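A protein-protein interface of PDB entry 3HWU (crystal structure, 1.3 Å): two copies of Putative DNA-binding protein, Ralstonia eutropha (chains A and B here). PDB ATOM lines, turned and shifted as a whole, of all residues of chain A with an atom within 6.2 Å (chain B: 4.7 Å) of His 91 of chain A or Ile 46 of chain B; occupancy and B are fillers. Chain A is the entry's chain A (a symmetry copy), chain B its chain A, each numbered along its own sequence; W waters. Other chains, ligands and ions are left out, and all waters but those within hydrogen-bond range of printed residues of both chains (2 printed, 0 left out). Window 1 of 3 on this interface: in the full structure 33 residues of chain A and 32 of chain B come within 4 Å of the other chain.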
ATOM      1  N   PHE A  43       4.564 -23.433 -12.886  1.00  0.00           N
ATOM      2  CA  PHE A  43       5.797 -24.179 -12.718  1.00  0.00           C
ATOM      3  C   PHE A  43       5.748 -25.142 -11.565  1.00  0.00           C
ATOM      4  O   PHE A  43       4.974 -24.977 -10.624  1.00  0.00           O
ATOM      5  CB  PHE A  43       7.019 -23.220 -12.600  1.00  0.00           C
ATOM      6  CG  PHE A  43       6.972 -22.249 -11.448  1.00  0.00           C
ATOM      7  CD1 PHE A  43       7.397 -22.607 -10.199  1.00  0.00           C
ATOM      8  CD2 PHE A  43       6.502 -20.958 -11.606  1.00  0.00           C
ATOM      9  CE1 PHE A  43       7.320 -21.733  -9.130  1.00  0.00           C
ATOM     10  CE2 PHE A  43       6.450 -20.088 -10.556  1.00  0.00           C
ATOM     11  CZ  PHE A  43       6.878 -20.478  -9.305  1.00  0.00           C
ATOM     12  N   THR A  78       5.573 -25.591  -6.273  1.00  0.00           N
ATOM     13  CA  THR A  78       4.505 -25.447  -7.253  1.00  0.00           C
ATOM     14  C   THR A  78       4.141 -23.976  -7.252  1.00  0.00           C
ATOM     15  O   THR A  78       3.990 -23.385  -6.186  1.00  0.00           O
ATOM     16  CB  THR A  78       3.284 -26.323  -6.891  1.00  0.00           C
ATOM     17  OG1 THR A  78       3.703 -27.686  -6.768  1.00  0.00           O
ATOM     18  CG2 THR A  78       2.196 -26.266  -7.956  1.00  0.00           C
ATOM     19  N   GLY A  79       3.953 -23.358  -8.421  1.00  0.00           N
ATOM     20  CA  GLY A  79       3.627 -21.934  -8.460  1.00  0.00           C
ATOM     21  C   GLY A  79       3.244 -21.392  -9.807  1.00  0.00           C
ATOM     22  O   GLY A  79       3.014 -22.165 -10.748  1.00  0.00           O
ATOM     23  N   SER A  80       3.102 -20.084  -9.871  1.00  0.00           N
ATOM     24  CA  SER A  80       2.757 -19.375 -11.096  1.00  0.00           C
ATOM     25  C   SER A  80       3.544 -18.100 -11.245  1.00  0.00           C
ATOM     26  O   SER A  80       3.970 -17.474 -10.278  1.00  0.00           O
ATOM     27  CB  SER A  80       1.264 -19.057 -11.169  1.00  0.00           C
ATOM     28  OG  SER A  80       0.852 -18.243 -10.087  1.00  0.00           O
ATOM     29  N   ILE A  81       3.719 -17.721 -12.519  1.00  0.00           N
ATOM     30  CA  ILE A  81       4.270 -16.414 -12.931  1.00  0.00           C
ATOM     31  C   ILE A  81       3.158 -15.572 -13.502  1.00  0.00           C
ATOM     32  O   ILE A  81       2.433 -16.008 -14.413  1.00  0.00           O
ATOM     33  CB  ILE A  81       5.352 -16.565 -14.008  1.00  0.00           C
ATOM     34  CG1 ILE A  81       6.488 -17.484 -13.508  1.00  0.00           C
ATOM     35  CG2 ILE A  81       5.936 -15.211 -14.422  1.00  0.00           C
ATOM     36  CD1 ILE A  81       7.651 -17.729 -14.531  1.00  0.00           C
ATOM     37  N   ALA A  82       3.009 -14.366 -12.964  1.00  0.00           N
ATOM     38  CA  ALA A  82       2.109 -13.366 -13.489  1.00  0.00           C
ATOM     39  C   ALA A  82       2.736 -11.998 -13.180  1.00  0.00           C
ATOM     40  O   ALA A  82       3.939 -11.911 -12.939  1.00  0.00           O
ATOM     41  CB  ALA A  82       0.681 -13.533 -12.957  1.00  0.00           C
ATOM     42  N   SER A  89       5.293 -11.071 -10.715  1.00  0.00           N
ATOM     43  CA  SER A  89       4.633 -11.430  -9.468  1.00  0.00           C
ATOM     44  C   SER A  89       4.569 -12.935  -9.367  1.00  0.00           C
ATOM     45  O   SER A  89       3.770 -13.587 -10.049  1.00  0.00           O
ATOM     46  CB  SER A  89       3.234 -10.839  -9.418  1.00  0.00           C
ATOM     47  OG  SER A  89       2.551 -11.197  -8.239  1.00  0.00           O
ATOM     48  N   ILE A  90       5.545 -13.496  -8.638  1.00  0.00           N
ATOM     49  CA  ILE A  90       5.685 -14.954  -8.513  1.00  0.00           C
ATOM     50  C   ILE A  90       4.867 -15.383  -7.291  1.00  0.00           C
ATOM     51  O   ILE A  90       4.963 -14.812  -6.200  1.00  0.00           O
ATOM     52  CB  ILE A  90       7.174 -15.372  -8.343  1.00  0.00           C
ATOM     53  CG1 ILE A  90       8.098 -14.820  -9.411  1.00  0.00           C
ATOM     54  CG2 ILE A  90       7.342 -16.877  -8.315  1.00  0.00           C
ATOM     55  CD1 ILE A  90       7.720 -15.121 -10.830  1.00  0.00           C
ATOM     56  N   HIS A  91       4.079 -16.430  -7.439  1.00  0.00           N
ATOM     57  CA  HIS A  91       3.291 -17.022  -6.373  1.00  0.00           C
ATOM     58  C   HIS A  91       3.752 -18.451  -6.282  1.00  0.00           C
ATOM     59  O   HIS A  91       3.528 -19.247  -7.203  1.00  0.00           O
ATOM     60  CB  HIS A  91       1.804 -16.980  -6.704  1.00  0.00           C
ATOM     61  CG  HIS A  91       0.939 -17.527  -5.640  1.00  0.00           C
ATOM     62  ND1 HIS A  91      -0.375 -17.897  -5.847  1.00  0.00           N
ATOM     63  CD2 HIS A  91       1.202 -17.766  -4.335  1.00  0.00           C
ATOM     64  CE1 HIS A  91      -0.887 -18.306  -4.699  1.00  0.00           C
ATOM     65  NE2 HIS A  91       0.052 -18.232  -3.766  1.00  0.00           N
ATOM     66  N   ALA A  92       4.449 -18.800  -5.207  1.00  0.00           N
ATOM     67  CA  ALA A  92       5.036 -20.113  -5.104  1.00  0.00           C
ATOM     68  C   ALA A  92       4.799 -20.688  -3.697  1.00  0.00           C
ATOM     69  O   ALA A  92       4.923 -19.981  -2.695  1.00  0.00           O
ATOM     70  CB  ALA A  92       6.562 -20.082  -5.397  1.00  0.00           C
ATOM     71  N   HIS A  93       4.562 -21.992  -3.662  1.00  0.00           N
ATOM     72  CA  HIS A  93       4.526 -22.770  -2.430  1.00  0.00           C
ATOM     73  C   HIS A  93       5.620 -23.837  -2.520  1.00  0.00           C
ATOM     74  O   HIS A  93       6.017 -24.269  -3.617  1.00  0.00           O
ATOM     75  CB  HIS A  93       3.161 -23.439  -2.216  1.00  0.00           C
ATOM     76  CG  HIS A  93       2.032 -22.491  -1.940  1.00  0.00           C
ATOM     77  ND1 HIS A  93       0.789 -22.940  -1.565  1.00  0.00           N
ATOM     78  CD2 HIS A  93       1.939 -21.143  -1.965  1.00  0.00           C
ATOM     79  CE1 HIS A  93       0.015 -21.906  -1.307  1.00  0.00           C
ATOM     80  NE2 HIS A  93       0.692 -20.802  -1.517  1.00  0.00           N
ATOM     81  N   HIS A 107       3.550 -21.205   1.893  1.00  0.00           N
ATOM     82  CA  HIS A 107       3.775 -20.062   1.005  1.00  0.00           C
ATOM     83  C   HIS A 107       5.219 -19.576   1.116  1.00  0.00           C
ATOM     84  O   HIS A 107       5.668 -19.212   2.202  1.00  0.00           O
ATOM     85  CB  HIS A 107       2.800 -18.946   1.426  1.00  0.00           C
ATOM     86  CG  HIS A 107       2.942 -17.675   0.668  1.00  0.00           C
ATOM     87  ND1 HIS A 107       2.015 -17.264  -0.260  1.00  0.00           N
ATOM     88  CD2 HIS A 107       3.860 -16.691   0.760  1.00  0.00           C
ATOM     89  CE1 HIS A 107       2.403 -16.103  -0.763  1.00  0.00           C
ATOM     90  NE2 HIS A 107       3.529 -15.740  -0.173  1.00  0.00           N
ATOM     91  N   ARG A 131      -2.128 -10.142 -11.277  1.00  0.00           N
ATOM     92  CA  ARG A 131      -2.717 -10.439  -9.997  1.00  0.00           C
ATOM     93  C   ARG A 131      -3.326  -9.157  -9.470  1.00  0.00           C
ATOM     94  O   ARG A 131      -2.823  -8.048  -9.755  1.00  0.00           O
ATOM     95  CB  ARG A 131      -1.648 -10.860  -9.002  1.00  0.00           C
ATOM     96  CG  ARG A 131      -0.925 -12.049  -9.332  1.00  0.00           C
ATOM     97  CD  ARG A 131      -0.154 -12.721  -8.077  1.00  0.00           C
ATOM     98  NE  ARG A 131       0.806 -13.587  -8.665  1.00  0.00           N
ATOM     99  CZ  ARG A 131       0.546 -14.845  -9.043  1.00  0.00           C
ATOM    100  NH1 ARG A 131      -0.589 -15.439  -8.718  1.00  0.00           N
ATOM    101  NH2 ARG A 131       1.435 -15.486  -9.762  1.00  0.00           N
ATOM    102  N   ASN A 140      -4.117 -11.201  -2.658  1.00  0.00           N
ATOM    103  CA  ASN A 140      -3.837 -11.228  -4.090  1.00  0.00           C
ATOM    104  C   ASN A 140      -4.383 -12.498  -4.732  1.00  0.00           C
ATOM    105  O   ASN A 140      -4.153 -13.573  -4.196  1.00  0.00           O
ATOM    106  CB  ASN A 140      -2.334 -11.146  -4.366  1.00  0.00           C
ATOM    107  CG  ASN A 140      -1.777  -9.785  -4.112  1.00  0.00           C
ATOM    108  OD1 ASN A 140      -0.814  -9.629  -3.344  1.00  0.00           O
ATOM    109  ND2 ASN A 140      -2.367  -8.787  -4.719  1.00  0.00           N
ATOM    110  N   GLY B  45      -1.665 -28.100  -8.459  1.00  0.00           N
ATOM    111  CA  GLY B  45      -2.201 -26.848  -7.998  1.00  0.00           C
ATOM    112  C   GLY B  45      -1.706 -26.423  -6.628  1.00  0.00           C
ATOM    113  O   GLY B  45      -1.001 -27.179  -5.964  1.00  0.00           O
ATOM    114  N   ILE B  46      -2.086 -25.196  -6.242  1.00  0.00           N
ATOM    115  CA  ILE B  46      -1.758 -24.609  -4.944  1.00  0.00           C
ATOM    116  C   ILE B  46      -2.949 -23.762  -4.525  1.00  0.00           C
ATOM    117  O   ILE B  46      -3.810 -23.418  -5.340  1.00  0.00           O
ATOM    118  CB  ILE B  46      -0.500 -23.702  -4.940  1.00  0.00           C
ATOM    119  CG1 ILE B  46      -0.587 -22.568  -5.985  1.00  0.00           C
ATOM    120  CG2 ILE B  46       0.746 -24.538  -5.128  1.00  0.00           C
ATOM    121  CD1 ILE B  46       0.487 -21.485  -5.860  1.00  0.00           C
ATOM    122  N   GLY B  47      -3.025 -23.436  -3.237  1.00  0.00           N
ATOM    123  CA  GLY B  47      -4.034 -22.457  -2.798  1.00  0.00           C
ATOM    124  C   GLY B  47      -4.139 -22.388  -1.296  1.00  0.00           C
ATOM    125  O   GLY B  47      -3.257 -22.893  -0.620  1.00  0.00           O
ATOM    126  N   MET B  74      -2.266 -24.918   1.004  1.00  0.00           N
ATOM    127  CA  MET B  74      -2.037 -26.123   0.247  1.00  0.00           C
ATOM    128  C   MET B  74      -0.782 -25.977  -0.592  1.00  0.00           C
ATOM    129  O   MET B  74      -0.732 -25.230  -1.579  1.00  0.00           O
ATOM    130  CB  MET B  74      -3.222 -26.450  -0.638  1.00  0.00           C
ATOM    131  CG  MET B  74      -3.066 -27.793  -1.306  1.00  0.00           C
ATOM    132  SD  MET B  74      -4.580 -28.413  -2.245  1.00  0.00           S
ATOM    133  CE  MET B  74      -4.424 -27.153  -3.808  1.00  0.00           C
ATOM    134  N   ALA B  75       0.283 -26.573  -0.071  1.00  0.00           N
ATOM    135  CA  ALA B  75       1.605 -26.454  -0.662  1.00  0.00           C
ATOM    136  C   ALA B  75       1.698 -27.122  -2.038  1.00  0.00           C
ATOM    137  O   ALA B  75       2.442 -26.692  -2.899  1.00  0.00           O
ATOM    138  CB  ALA B  75       2.683 -27.034   0.306  1.00  0.00           C
ATOM    139  N   ASN B  76       0.900 -28.181  -2.232  1.00  0.00           N
ATOM    140  CA  ASN B  76       0.769 -28.822  -3.541  1.00  0.00           C
ATOM    141  C   ASN B  76      -0.452 -29.686  -3.558  1.00  0.00           C
ATOM    142  O   ASN B  76      -0.771 -30.288  -2.545  1.00  0.00           O
ATOM    143  CB  ASN B  76       2.018 -29.691  -3.841  1.00  0.00           C
ATOM    144  CG  ASN B  76       1.791 -30.572  -5.061  1.00  0.00           C
ATOM    145  OD1 ASN B  76       1.299 -31.718  -4.904  1.00  0.00           O
ATOM    146  ND2 ASN B  76       2.099 -30.070  -6.298  1.00  0.00           N
ATOM    147  N   SER B 117      -7.339 -18.267  -2.857  1.00  0.00           N
ATOM    148  CA  SER B 117      -7.702 -18.804  -4.181  1.00  0.00           C
ATOM    149  C   SER B 117      -7.084 -20.187  -4.337  1.00  0.00           C
ATOM    150  O   SER B 117      -6.361 -20.643  -3.442  1.00  0.00           O
ATOM    151  CB  SER B 117      -7.215 -17.863  -5.289  1.00  0.00           C
ATOM    152  OG  SER B 117      -5.822 -17.703  -5.247  1.00  0.00           O
ATOM    153  N   CYS B 118      -7.331 -20.837  -5.459  1.00  0.00           N
ATOM    154  CA  CYS B 118      -6.671 -22.093  -5.799  1.00  0.00           C
ATOM    155  C   CYS B 118      -6.346 -22.040  -7.288  1.00  0.00           C
ATOM    156  O   CYS B 118      -7.266 -21.925  -8.105  1.00  0.00           O
ATOM    157  CB  CYS B 118      -7.557 -23.301  -5.423  1.00  0.00           C
ATOM    158  SG  CYS B 118      -6.886 -24.872  -5.911  1.00  0.00           S
ATOM    159  N   GLU B 119      -5.061 -22.135  -7.628  1.00  0.00           N
ATOM    160  CA  GLU B 119      -4.565 -22.150  -8.999  1.00  0.00           C
ATOM    161  C   GLU B 119      -4.352 -23.603  -9.391  1.00  0.00           C
ATOM    162  O   GLU B 119      -3.681 -24.328  -8.667  1.00  0.00           O
ATOM    163  CB  GLU B 119      -3.247 -21.401  -9.126  1.00  0.00           C
ATOM    164  CG  GLU B 119      -3.325 -19.932  -8.739  1.00  0.00           C
ATOM    165  CD  GLU B 119      -1.983 -19.229  -8.685  1.00  0.00           C
ATOM    166  OE1 GLU B 119      -0.973 -19.841  -9.056  1.00  0.00           O
ATOM    167  OE2 GLU B 119      -1.970 -18.046  -8.292  1.00  0.00           O
HETATM  168  O   HOH W   1      -5.302 -15.824  -3.382  1.00  0.00           O
HETATM  169  O   HOH W   2       0.077 -22.447  -9.751  1.00  0.00           O
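The backbone carbonyl oxygen (O) of Met 74 of chain B lies within hydrogen-bond range of a ring nitrogen (ND1) of His 93 of chain A (2.7 Å). The side-chain amide nitrogen (ND2) of Asn 76 of chain B lies within hydrogen-bond range of the side-chain hydroxyl (OG1) of Thr 78 of chain A, at 2.9 Å. The side-chain carboxylate (OE1) of Glu 119 of chain B is in hydrogen-bond range of the side-chain hydroxyl (OG) of Ser 80 of chain A. ND1 of His 91 of chain A lies within hydrogen-bond range of OE2 of Glu 119 of chain B. OE2 of Glu 119 of chain B lies within salt-bridge range of NH1 of Arg 131 of chain A, 3.0 Å away.
The backbone carbonyl oxygen of Ile 46 of chain B sits at hydrogen-bond distance from the backbone NH of Glu 119 of chain B. The backbone carbonyl oxygen (O) of Thr 78 of chain A lies within hydrogen-bond range of the backbone NH (N) of His 93 of chain A, at 2.9 Å. The backbone NH of Ser 80 of chain A is in hydrogen-bond range of the backbone carbonyl oxygen of His 91 of chain A (2.8 Å). NH2 of Arg 131 of chain A is in hydrogen-bond range of OG of Ser 80 of chain A. The guanidinium group of Arg 131 of chain A is in hydrogen-bond range of the side-chain hydroxyl of Ser 89 of chain A (3.0 Å). A ring nitrogen (NE2) of His 91 of chain A sits at hydrogen-bond distance from a ring nitrogen (NE2) of His 93 of chain A.
O of Gly 45 of chain B touches CG2 of Thr 78 of chain A (3.9 Å). CB of Thr 78 of chain A touches CG2 of Ile 46 of chain B, at 3.6 Å. His 91 of chain A touches Ile 46 of chain B (CE1 to CD1, 3.7 Å). His 93 of chain A touches Ile 46 of chain B. Gly 47 of chain B touches His 93 of chain A (O to CE1, 3.5 Å). O of Ala 75 of chain B touches CB of His 93 of chain A, at 3.4 Å.
Of chain B, only Ile 46 and Glu 119 come within 4 Å of His 91 of chain A. Ile 46 of chain B touches just these residues of chain A: Thr 78, His 91 and His 93. Of the printed residues of chain A, Asn 76 of chain B touches Thr 78 (2.9 Å). Printed residues of chain A within 4 Å of Gly 47 of chain B: His 93. Of the printed residues of chain A, Glu 119 of chain B touches Ser 80 (2.6 Å), His 91 (2.9 Å) and Arg 131 (3.0 Å). Printed residues of chain B within 4 Å of His 93 of chain A: Ile 46, Gly 47, Met 74 and Ala 75. Of the printed residues of chain A, Ala 75 of chain B touches His 93. Ile 90 of chain A touches none of the printed residues of chain B. Gly 79 of chain A touches none of the printed residues of chain B.
Hydrophobic or aromatic side chains of chain B that line the printed part of chain A: Ile 46. Among the printed residues, 11 pairs touch across the chains. Among the printed residues, Asp or Glu carboxylates within 4 Å of a Lys or Arg side-chain nitrogen of the other chain: Arg 131 of chain A with Glu 119 of chain B.
No position is printed for both chains. Of the 11 pairs that touch across the chains among the printed residues, none has its exchanged pair printed and touching as well.
Water W1 bridges O of Asn 140 of chain A and OG of Ser 117 of chain B. Water W2 lies within hydrogen-bond range of the side-chain carboxylate (OE1) of Glu 119 of chain B (2.9 Å) and the backbone carbonyl oxygen (O) of Gly 79 of chain A (3.1 Å).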
